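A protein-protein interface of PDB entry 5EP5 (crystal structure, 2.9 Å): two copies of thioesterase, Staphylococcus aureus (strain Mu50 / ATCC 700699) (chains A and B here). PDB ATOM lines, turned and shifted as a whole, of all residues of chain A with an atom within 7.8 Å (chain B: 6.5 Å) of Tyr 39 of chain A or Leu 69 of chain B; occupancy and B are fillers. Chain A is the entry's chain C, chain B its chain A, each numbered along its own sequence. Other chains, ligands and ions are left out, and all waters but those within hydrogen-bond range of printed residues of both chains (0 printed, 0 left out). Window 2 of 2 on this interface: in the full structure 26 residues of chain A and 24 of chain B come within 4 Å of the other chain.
The backbone carbonyl oxygen of Leu 69 of chain B is in hydrogen-bond range of the backbone NH of Ala 122 of chain B, at 2.7 Å.
The backbone NH (N) of Ile 67 of chain B sits at hydrogen-bond distance from the backbone carbonyl oxygen (O) of Lys 124 of chain B, 2.8 Å away.
N of Leu 71 of chain B sits at hydrogen-bond distance from O of Thr 120 of chain B, at 2.8 Å.
Gln 35 of chain A touches Leu 69 of chain B.
Ile 67 of chain B touches Phe 37 of chain A (CG1 to CD1, 3.7 Å).
Phe 37 of chain A touches Pro 68 of chain B.
Tyr 39 of chain A touches Leu 69 of chain B.
His 77 of chain A touches Gly 70 of chain B.
O of Leu 71 of chain B is in hydrogen-bond range of N of His 77 of chain A.
Hydrophobic or aromatic side chains of chain B that line the printed part of chain A: Ile 67, Pro 68, Leu 69 and Leu 71.
Of the 21 printed residues of chain A, 4 touch a printed residue of chain B.
Hydrophobic or aromatic side chains of chain A that line the printed part of chain B: Phe 37, Tyr 39 and His 77.
Among the printed residues, 6 pairs touch across the chains.
No position is printed for both chains.
Of the 6 pairs that touch across the chains among the printed residues, none has its exchanged pair printed and touching as well.
Of chain B, only Leu 69 comes within 4 Å of Tyr 39 of chain A.
Leu 69 of chain B touches just these residues of chain A: Gln 35 (3.98 Å) and Tyr 39 (3.9 Å).
Printed residues of chain A within 4 Å of Gly 70 of chain B: His 77 (3.1 Å).
Of the printed residues of chain A, Ile 67 of chain B touches Phe 37.
Of the printed residues of chain B, Gln 35 of chain A touches Leu 69.
Of the printed residues of chain A, Pro 68 of chain B touches Phe 37.
Of the printed residues of chain A, Leu 71 of chain B touches His 77 (2.8 Å).
The nearest residue of chain A that does not touch Leu 69 of chain B is Ser 80 of chain A (4.6 Å).
The nearest printed residue of chain B that does not touch His 77 of chain A is Met 73 of chain B (4.1 Å).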
ATOM      1  N   VAL A  29     -12.227  27.004 -15.024  1.00  0.00           N
ATOM      2  CA  VAL A  29     -13.500  27.377 -14.441  1.00  0.00           C
ATOM      3  C   VAL A  29     -13.301  27.618 -12.953  1.00  0.00           C
ATOM      4  O   VAL A  29     -13.264  26.679 -12.179  1.00  0.00           O
ATOM      5  CB  VAL A  29     -14.540  26.266 -14.638  1.00  0.00           C
ATOM      6  CG1 VAL A  29     -15.862  26.621 -13.944  1.00  0.00           C
ATOM      7  CG2 VAL A  29     -14.737  26.012 -16.126  1.00  0.00           C
ATOM      8  N   THR A  30     -13.149  28.881 -12.574  1.00  0.00           N
ATOM      9  CA  THR A  30     -12.984  29.279 -11.182  1.00  0.00           C
ATOM     10  C   THR A  30     -14.196  30.044 -10.686  1.00  0.00           C
ATOM     11  O   THR A  30     -15.087  30.383 -11.470  1.00  0.00           O
ATOM     12  CB  THR A  30     -11.717  30.132 -10.999  1.00  0.00           C
ATOM     13  OG1 THR A  30     -11.888  31.434 -11.594  1.00  0.00           O
ATOM     14  CG2 THR A  30     -10.517  29.405 -11.614  1.00  0.00           C
ATOM     15  N   ASP A  31     -14.236  30.306  -9.374  1.00  0.00           N
ATOM     16  CA  ASP A  31     -15.356  31.048  -8.789  1.00  0.00           C
ATOM     17  C   ASP A  31     -15.427  32.447  -9.373  1.00  0.00           C
ATOM     18  O   ASP A  31     -16.521  32.951  -9.576  1.00  0.00           O
ATOM     19  CB  ASP A  31     -15.278  31.140  -7.259  1.00  0.00           C
ATOM     20  CG  ASP A  31     -15.516  29.813  -6.570  1.00  0.00           C
ATOM     21  OD1 ASP A  31     -16.229  28.925  -7.116  1.00  0.00           O
ATOM     22  OD2 ASP A  31     -14.980  29.665  -5.457  1.00  0.00           O
ATOM     23  N   VAL A  33     -15.141  33.421 -12.317  1.00  0.00           N
ATOM     24  CA  VAL A  33     -15.897  33.405 -13.580  1.00  0.00           C
ATOM     25  C   VAL A  33     -17.211  32.631 -13.479  1.00  0.00           C
ATOM     26  O   VAL A  33     -17.797  32.296 -14.492  1.00  0.00           O
ATOM     27  CB  VAL A  33     -15.084  32.818 -14.758  1.00  0.00           C
ATOM     28  CG1 VAL A  33     -14.009  33.782 -15.221  1.00  0.00           C
ATOM     29  CG2 VAL A  33     -14.489  31.467 -14.403  1.00  0.00           C
ATOM     30  N   LYS A  34     -17.697  32.365 -12.271  1.00  0.00           N
ATOM     31  CA  LYS A  34     -18.963  31.615 -12.091  1.00  0.00           C
ATOM     32  C   LYS A  34     -20.167  32.535 -11.967  1.00  0.00           C
ATOM     33  O   LYS A  34     -20.032  33.704 -11.636  1.00  0.00           O
ATOM     34  CB  LYS A  34     -18.908  30.689 -10.866  1.00  0.00           C
ATOM     35  CG  LYS A  34     -18.119  29.406 -11.086  1.00  0.00           C
ATOM     36  CD  LYS A  34     -18.160  28.496  -9.876  1.00  0.00           C
ATOM     37  CE  LYS A  34     -17.448  27.181 -10.125  1.00  0.00           C
ATOM     38  NZ  LYS A  34     -17.528  26.316  -8.923  1.00  0.00           N
ATOM     39  N   GLN A  35     -21.344  31.997 -12.262  1.00  0.00           N
ATOM     40  CA  GLN A  35     -22.610  32.659 -11.924  1.00  0.00           C
ATOM     41  C   GLN A  35     -22.813  32.350 -10.445  1.00  0.00           C
ATOM     42  O   GLN A  35     -22.109  31.487  -9.920  1.00  0.00           O
ATOM     43  CB  GLN A  35     -23.781  32.122 -12.766  1.00  0.00           C
ATOM     44  CG  GLN A  35     -24.198  30.707 -12.371  1.00  0.00           C
ATOM     45  CD  GLN A  35     -25.376  30.145 -13.144  1.00  0.00           C
ATOM     46  OE1 GLN A  35     -25.887  30.782 -14.061  1.00  0.00           O
ATOM     47  NE2 GLN A  35     -25.820  28.942 -12.771  1.00  0.00           N
ATOM     48  N   PRO A  36     -23.775  33.012  -9.769  1.00  0.00           N
ATOM     49  CA  PRO A  36     -23.942  32.741  -8.323  1.00  0.00           C
ATOM     50  C   PRO A  36     -24.309  31.288  -7.909  1.00  0.00           C
ATOM     51  O   PRO A  36     -23.879  30.807  -6.853  1.00  0.00           O
ATOM     52  CB  PRO A  36     -25.071  33.690  -7.923  1.00  0.00           C
ATOM     53  CG  PRO A  36     -25.004  34.803  -8.905  1.00  0.00           C
ATOM     54  CD  PRO A  36     -24.557  34.192 -10.197  1.00  0.00           C
ATOM     55  N   PHE A  37     -25.069  30.610  -8.758  1.00  0.00           N
ATOM     56  CA  PHE A  37     -25.711  29.324  -8.425  1.00  0.00           C
ATOM     57  C   PHE A  37     -24.841  28.175  -7.900  1.00  0.00           C
ATOM     58  O   PHE A  37     -25.183  27.600  -6.874  1.00  0.00           O
ATOM     59  CB  PHE A  37     -26.589  28.845  -9.581  1.00  0.00           C
ATOM     60  CG  PHE A  37     -27.731  29.789  -9.871  1.00  0.00           C
ATOM     61  CD1 PHE A  37     -28.950  29.716  -9.153  1.00  0.00           C
ATOM     62  CD2 PHE A  37     -27.568  30.817 -10.788  1.00  0.00           C
ATOM     63  CE1 PHE A  37     -29.969  30.635  -9.387  1.00  0.00           C
ATOM     64  CE2 PHE A  37     -28.586  31.726 -11.032  1.00  0.00           C
ATOM     65  CZ  PHE A  37     -29.784  31.643 -10.326  1.00  0.00           C
ATOM     66  N   GLY A  38     -23.727  27.832  -8.537  1.00  0.00           N
ATOM     67  CA  GLY A  38     -23.139  28.563  -9.638  1.00  0.00           C
ATOM     68  C   GLY A  38     -22.288  27.728 -10.572  1.00  0.00           C
ATOM     69  O   GLY A  38     -21.405  26.985 -10.158  1.00  0.00           O
ATOM     70  N   TYR A  39     -22.612  27.844 -11.850  1.00  0.00           N
ATOM     71  CA  TYR A  39     -21.868  27.267 -12.942  1.00  0.00           C
ATOM     72  C   TYR A  39     -20.971  28.341 -13.551  1.00  0.00           C
ATOM     73  O   TYR A  39     -20.999  29.512 -13.138  1.00  0.00           O
ATOM     74  CB  TYR A  39     -22.859  26.780 -14.003  1.00  0.00           C
ATOM     75  CG  TYR A  39     -23.898  25.786 -13.497  1.00  0.00           C
ATOM     76  CD1 TYR A  39     -23.505  24.595 -12.855  1.00  0.00           C
ATOM     77  CD2 TYR A  39     -25.266  26.010 -13.690  1.00  0.00           C
ATOM     78  CE1 TYR A  39     -24.448  23.680 -12.398  1.00  0.00           C
ATOM     79  CE2 TYR A  39     -26.209  25.101 -13.236  1.00  0.00           C
ATOM     80  CZ  TYR A  39     -25.799  23.944 -12.595  1.00  0.00           C
ATOM     81  OH  TYR A  39     -26.743  23.055 -12.165  1.00  0.00           O
ATOM     82  N   LEU A  40     -20.188  27.948 -14.551  1.00  0.00           N
ATOM     83  CA  LEU A  40     -19.496  28.914 -15.389  1.00  0.00           C
ATOM     84  C   LEU A  40     -20.516  29.921 -15.940  1.00  0.00           C
ATOM     85  O   LEU A  40     -21.582  29.539 -16.425  1.00  0.00           O
ATOM     86  CB  LEU A  40     -18.786  28.193 -16.530  1.00  0.00           C
ATOM     87  CG  LEU A  40     -18.045  29.046 -17.551  1.00  0.00           C
ATOM     88  CD1 LEU A  40     -17.005  29.921 -16.889  1.00  0.00           C
ATOM     89  CD2 LEU A  40     -17.397  28.135 -18.574  1.00  0.00           C
ATOM     90  N   HIS A  41     -20.205  31.207 -15.819  1.00  0.00           N
ATOM     91  CA  HIS A  41     -21.094  32.292 -16.292  1.00  0.00           C
ATOM     92  C   HIS A  41     -21.154  32.245 -17.810  1.00  0.00           C
ATOM     93  O   HIS A  41     -20.138  32.098 -18.445  1.00  0.00           O
ATOM     94  CB  HIS A  41     -20.539  33.632 -15.807  1.00  0.00           C
ATOM     95  CG  HIS A  41     -21.486  34.783 -15.886  1.00  0.00           C
ATOM     96  ND1 HIS A  41     -21.822  35.366 -17.079  1.00  0.00           N
ATOM     97  CD2 HIS A  41     -22.073  35.535 -14.923  1.00  0.00           C
ATOM     98  CE1 HIS A  41     -22.605  36.407 -16.861  1.00  0.00           C
ATOM     99  NE2 HIS A  41     -22.780  36.528 -15.558  1.00  0.00           N
ATOM    100  N   GLY A  42     -22.350  32.325 -18.373  1.00  0.00           N
ATOM    101  CA  GLY A  42     -22.535  32.235 -19.809  1.00  0.00           C
ATOM    102  C   GLY A  42     -21.780  33.331 -20.523  1.00  0.00           C
ATOM    103  O   GLY A  42     -21.171  33.103 -21.567  1.00  0.00           O
ATOM    104  N   ALA A  44     -19.006  34.671 -19.538  1.00  0.00           N
ATOM    105  CA  ALA A  44     -17.569  34.398 -19.487  1.00  0.00           C
ATOM    106  C   ALA A  44     -17.185  33.463 -20.624  1.00  0.00           C
ATOM    107  O   ALA A  44     -16.156  33.653 -21.284  1.00  0.00           O
ATOM    108  CB  ALA A  44     -17.174  33.792 -18.150  1.00  0.00           C
ATOM    109  N   HIS A  77     -26.173  28.314 -25.336  1.00  0.00           N
ATOM    110  CA  HIS A  77     -25.662  27.612 -24.188  1.00  0.00           C
ATOM    111  C   HIS A  77     -26.353  26.246 -24.153  1.00  0.00           C
ATOM    112  O   HIS A  77     -27.578  26.179 -24.200  1.00  0.00           O
ATOM    113  CB  HIS A  77     -25.962  28.426 -22.943  1.00  0.00           C
ATOM    114  CG  HIS A  77     -25.252  29.747 -22.893  1.00  0.00           C
ATOM    115  ND1 HIS A  77     -23.881  29.851 -22.981  1.00  0.00           N
ATOM    116  CD2 HIS A  77     -25.713  31.010 -22.715  1.00  0.00           C
ATOM    117  CE1 HIS A  77     -23.528  31.121 -22.881  1.00  0.00           C
ATOM    118  NE2 HIS A  77     -24.621  31.844 -22.709  1.00  0.00           N
ATOM    119  N   ILE A  78     -25.559  25.175 -24.104  1.00  0.00           N
ATOM    120  CA  ILE A  78     -26.051  23.801 -24.205  1.00  0.00           C
ATOM    121  C   ILE A  78     -25.902  23.016 -22.894  1.00  0.00           C
ATOM    122  O   ILE A  78     -26.858  22.450 -22.405  1.00  0.00           O
ATOM    123  CB  ILE A  78     -25.284  23.001 -25.277  1.00  0.00           C
ATOM    124  CG1 ILE A  78     -25.144  23.769 -26.613  1.00  0.00           C
ATOM    125  CG2 ILE A  78     -25.913  21.622 -25.455  1.00  0.00           C
ATOM    126  CD1 ILE A  78     -26.433  24.158 -27.273  1.00  0.00           C
ATOM    127  N   HIS A  79     -24.687  22.924 -22.369  1.00  0.00           N
ATOM    128  CA  HIS A  79     -24.422  22.213 -21.119  1.00  0.00           C
ATOM    129  C   HIS A  79     -23.717  23.128 -20.138  1.00  0.00           C
ATOM    130  O   HIS A  79     -23.170  24.161 -20.525  1.00  0.00           O
ATOM    131  CB  HIS A  79     -23.547  20.983 -21.349  1.00  0.00           C
ATOM    132  CG  HIS A  79     -24.228  19.878 -22.081  1.00  0.00           C
ATOM    133  ND1 HIS A  79     -24.007  19.629 -23.417  1.00  0.00           N
ATOM    134  CD2 HIS A  79     -25.107  18.939 -21.661  1.00  0.00           C
ATOM    135  CE1 HIS A  79     -24.728  18.587 -23.793  1.00  0.00           C
ATOM    136  NE2 HIS A  79     -25.406  18.152 -22.747  1.00  0.00           N
ATOM    137  N   SER A  80     -23.724  22.720 -18.868  1.00  0.00           N
ATOM    138  CA  SER A  80     -23.107  23.478 -17.791  1.00  0.00           C
ATOM    139  C   SER A  80     -21.697  23.020 -17.567  1.00  0.00           C
ATOM    140  O   SER A  80     -21.331  21.913 -17.916  1.00  0.00           O
ATOM    141  CB  SER A  80     -23.915  23.354 -16.497  1.00  0.00           C
ATOM    142  OG  SER A  80     -25.189  23.959 -16.665  1.00  0.00           O
ATOM    143  N   ALA A  81     -20.906  23.917 -17.003  1.00  0.00           N
ATOM    144  CA  ALA A  81     -19.547  23.641 -16.581  1.00  0.00           C
ATOM    145  C   ALA A  81     -19.444  24.101 -15.144  1.00  0.00           C
ATOM    146  O   ALA A  81     -19.799  25.232 -14.808  1.00  0.00           O
ATOM    147  CB  ALA A  81     -18.554  24.395 -17.445  1.00  0.00           C
ATOM    148  N   LYS A  82     -18.999  23.200 -14.286  1.00  0.00           N
ATOM    149  CA  LYS A  82     -18.855  23.491 -12.877  1.00  0.00           C
ATOM    150  C   LYS A  82     -17.389  23.603 -12.443  1.00  0.00           C
ATOM    151  O   LYS A  82     -17.106  24.301 -11.476  1.00  0.00           O
ATOM    152  CB  LYS A  82     -19.598  22.425 -12.074  1.00  0.00           C
ATOM    153  CG  LYS A  82     -19.564  22.615 -10.563  1.00  0.00           C
ATOM    154  CD  LYS A  82     -20.005  24.010 -10.110  1.00  0.00           C
ATOM    155  CE  LYS A  82     -20.539  23.985  -8.680  1.00  0.00           C
ATOM    156  NZ  LYS A  82     -19.585  23.370  -7.711  1.00  0.00           N
ATOM    157  N   ASP A  83     -16.463  22.943 -13.146  1.00  0.00           N
ATOM    158  CA  ASP A  83     -15.056  22.975 -12.746  1.00  0.00           C
ATOM    159  C   ASP A  83     -14.110  22.542 -13.857  1.00  0.00           C
ATOM    160  O   ASP A  83     -14.533  22.217 -14.937  1.00  0.00           O
ATOM    161  CB  ASP A  83     -14.844  22.107 -11.485  1.00  0.00           C
ATOM    162  CG  ASP A  83     -15.253  20.662 -11.693  1.00  0.00           C
ATOM    163  OD1 ASP A  83     -14.946  20.095 -12.761  1.00  0.00           O
ATOM    164  OD2 ASP A  83     -15.880  20.084 -10.782  1.00  0.00           O
ATOM    165  N   ILE B  67     -34.542  27.581 -11.602  1.00  0.00           N
ATOM    166  CA  ILE B  67     -33.279  28.254 -11.861  1.00  0.00           C
ATOM    167  C   ILE B  67     -33.303  28.880 -13.264  1.00  0.00           C
ATOM    168  O   ILE B  67     -33.731  28.224 -14.235  1.00  0.00           O
ATOM    169  CB  ILE B  67     -32.086  27.284 -11.690  1.00  0.00           C
ATOM    170  CG1 ILE B  67     -30.771  28.023 -11.906  1.00  0.00           C
ATOM    171  CG2 ILE B  67     -32.187  26.077 -12.630  1.00  0.00           C
ATOM    172  CD1 ILE B  67     -29.561  27.130 -11.794  1.00  0.00           C
ATOM    173  N   PRO B  68     -32.840  30.136 -13.389  1.00  0.00           N
ATOM    174  CA  PRO B  68     -32.701  30.789 -14.704  1.00  0.00           C
ATOM    175  C   PRO B  68     -31.351  30.526 -15.344  1.00  0.00           C
ATOM    176  O   PRO B  68     -30.338  30.902 -14.770  1.00  0.00           O
ATOM    177  CB  PRO B  68     -32.815  32.270 -14.370  1.00  0.00           C
ATOM    178  CG  PRO B  68     -32.306  32.360 -12.973  1.00  0.00           C
ATOM    179  CD  PRO B  68     -32.457  31.036 -12.300  1.00  0.00           C
ATOM    180  N   LEU B  69     -31.336  29.878 -16.510  1.00  0.00           N
ATOM    181  CA  LEU B  69     -30.090  29.594 -17.239  1.00  0.00           C
ATOM    182  C   LEU B  69     -30.105  30.280 -18.592  1.00  0.00           C
ATOM    183  O   LEU B  69     -31.061  30.123 -19.372  1.00  0.00           O
ATOM    184  CB  LEU B  69     -29.903  28.092 -17.480  1.00  0.00           C
ATOM    185  CG  LEU B  69     -29.617  27.149 -16.307  1.00  0.00           C
ATOM    186  CD1 LEU B  69     -29.439  25.730 -16.861  1.00  0.00           C
ATOM    187  CD2 LEU B  69     -28.409  27.570 -15.464  1.00  0.00           C
ATOM    188  N   GLY B  70     -29.022  30.996 -18.886  1.00  0.00           N
ATOM    189  CA  GLY B  70     -28.845  31.607 -20.184  1.00  0.00           C
ATOM    190  C   GLY B  70     -28.940  30.518 -21.219  1.00  0.00           C
ATOM    191  O   GLY B  70     -28.273  29.517 -21.110  1.00  0.00           O
ATOM    192  N   LEU B  71     -29.812  30.696 -22.196  1.00  0.00           N
ATOM    193  CA  LEU B  71     -30.012  29.694 -23.228  1.00  0.00           C
ATOM    194  C   LEU B  71     -29.465  30.168 -24.566  1.00  0.00           C
ATOM    195  O   LEU B  71     -28.722  29.453 -25.233  1.00  0.00           O
ATOM    196  CB  LEU B  71     -31.498  29.359 -23.366  1.00  0.00           C
ATOM    197  CG  LEU B  71     -31.801  28.232 -24.365  1.00  0.00           C
ATOM    198  CD1 LEU B  71     -31.142  26.940 -23.907  1.00  0.00           C
ATOM    199  CD2 LEU B  71     -33.294  28.038 -24.565  1.00  0.00           C
ATOM    200  N   GLU B  72     -29.871  31.359 -24.981  1.00  0.00           N
ATOM    201  CA  GLU B  72     -29.334  31.974 -26.193  1.00  0.00           C
ATOM    202  C   GLU B  72     -29.002  33.454 -25.935  1.00  0.00           C
ATOM    203  O   GLU B  72     -29.708  34.125 -25.206  1.00  0.00           O
ATOM    204  CB  GLU B  72     -30.337  31.799 -27.333  1.00  0.00           C
ATOM    205  CG  GLU B  72     -29.725  31.661 -28.723  1.00  0.00           C
ATOM    206  CD  GLU B  72     -29.348  32.987 -29.392  1.00  0.00           C
ATOM    207  OE1 GLU B  72     -29.924  34.062 -29.040  1.00  0.00           O
ATOM    208  OE2 GLU B  72     -28.486  32.950 -30.310  1.00  0.00           O
ATOM    209  N   MET B  73     -27.901  33.949 -26.482  1.00  0.00           N
ATOM    210  CA  MET B  73     -27.572  35.380 -26.398  1.00  0.00           C
ATOM    211  C   MET B  73     -27.141  35.838 -27.769  1.00  0.00           C
ATOM    212  O   MET B  73     -26.394  35.145 -28.441  1.00  0.00           O
ATOM    213  CB  MET B  73     -26.404  35.650 -25.441  1.00  0.00           C
ATOM    214  CG  MET B  73     -26.636  35.229 -24.004  1.00  0.00           C
ATOM    215  SD  MET B  73     -27.711  36.368 -23.120  1.00  0.00           S
ATOM    216  CE  MET B  73     -28.478  35.218 -21.956  1.00  0.00           C
ATOM    217  N   THR B 120     -32.105  35.085 -24.213  1.00  0.00           N
ATOM    218  CA  THR B 120     -33.172  34.124 -23.966  1.00  0.00           C
ATOM    219  C   THR B 120     -32.701  33.302 -22.767  1.00  0.00           C
ATOM    220  O   THR B 120     -31.606  32.707 -22.800  1.00  0.00           O
ATOM    221  CB  THR B 120     -33.473  33.242 -25.212  1.00  0.00           C
ATOM    222  OG1 THR B 120     -33.850  34.077 -26.316  1.00  0.00           O
ATOM    223  CG2 THR B 120     -34.587  32.236 -24.925  1.00  0.00           C
ATOM    224  N   VAL B 121     -33.518  33.311 -21.712  1.00  0.00           N
ATOM    225  CA  VAL B 121     -33.199  32.659 -20.460  1.00  0.00           C
ATOM    226  C   VAL B 121     -34.175  31.508 -20.267  1.00  0.00           C
ATOM    227  O   VAL B 121     -35.398  31.688 -20.372  1.00  0.00           O
ATOM    228  CB  VAL B 121     -33.319  33.641 -19.279  1.00  0.00           C
ATOM    229  CG1 VAL B 121     -33.031  32.926 -17.954  1.00  0.00           C
ATOM    230  CG2 VAL B 121     -32.398  34.845 -19.482  1.00  0.00           C
ATOM    231  N   ALA B 122     -33.634  30.320 -20.007  1.00  0.00           N
ATOM    232  CA  ALA B 122     -34.466  29.147 -19.745  1.00  0.00           C
ATOM    233  C   ALA B 122     -34.805  29.144 -18.276  1.00  0.00           C
ATOM    234  O   ALA B 122     -33.957  29.440 -17.438  1.00  0.00           O
ATOM    235  CB  ALA B 122     -33.748  27.861 -20.117  1.00  0.00           C
ATOM    236  N   ILE B 123     -36.050  28.800 -17.972  1.00  0.00           N
ATOM    237  CA  ILE B 123     -36.482  28.595 -16.599  1.00  0.00           C
ATOM    238  C   ILE B 123     -36.589  27.091 -16.332  1.00  0.00           C
ATOM    239  O   ILE B 123     -37.512  26.423 -16.805  1.00  0.00           O
ATOM    240  CB  ILE B 123     -37.820  29.325 -16.341  1.00  0.00           C
ATOM    241  CG1 ILE B 123     -37.773  30.792 -16.820  1.00  0.00           C
ATOM    242  CG2 ILE B 123     -38.134  29.295 -14.859  1.00  0.00           C
ATOM    243  CD1 ILE B 123     -36.642  31.600 -16.231  1.00  0.00           C
ATOM    244  N   LYS B 124     -35.637  26.570 -15.563  1.00  0.00           N
ATOM    245  CA  LYS B 124     -35.500  25.125 -15.352  1.00  0.00           C
ATOM    246  C   LYS B 124     -35.850  24.693 -13.939  1.00  0.00           C
ATOM    247  O   LYS B 124     -35.533  25.400 -12.986  1.00  0.00           O
ATOM    248  CB  LYS B 124     -34.056  24.700 -15.543  1.00  0.00           C
ATOM    249  CG  LYS B 124     -33.450  24.994 -16.890  1.00  0.00           C
ATOM    250  CD  LYS B 124     -34.254  24.300 -17.977  1.00  0.00           C
ATOM    251  CE  LYS B 124     -33.389  24.008 -19.196  1.00  0.00           C
ATOM    252  NZ  LYS B 124     -33.896  22.807 -19.903  1.00  0.00           N
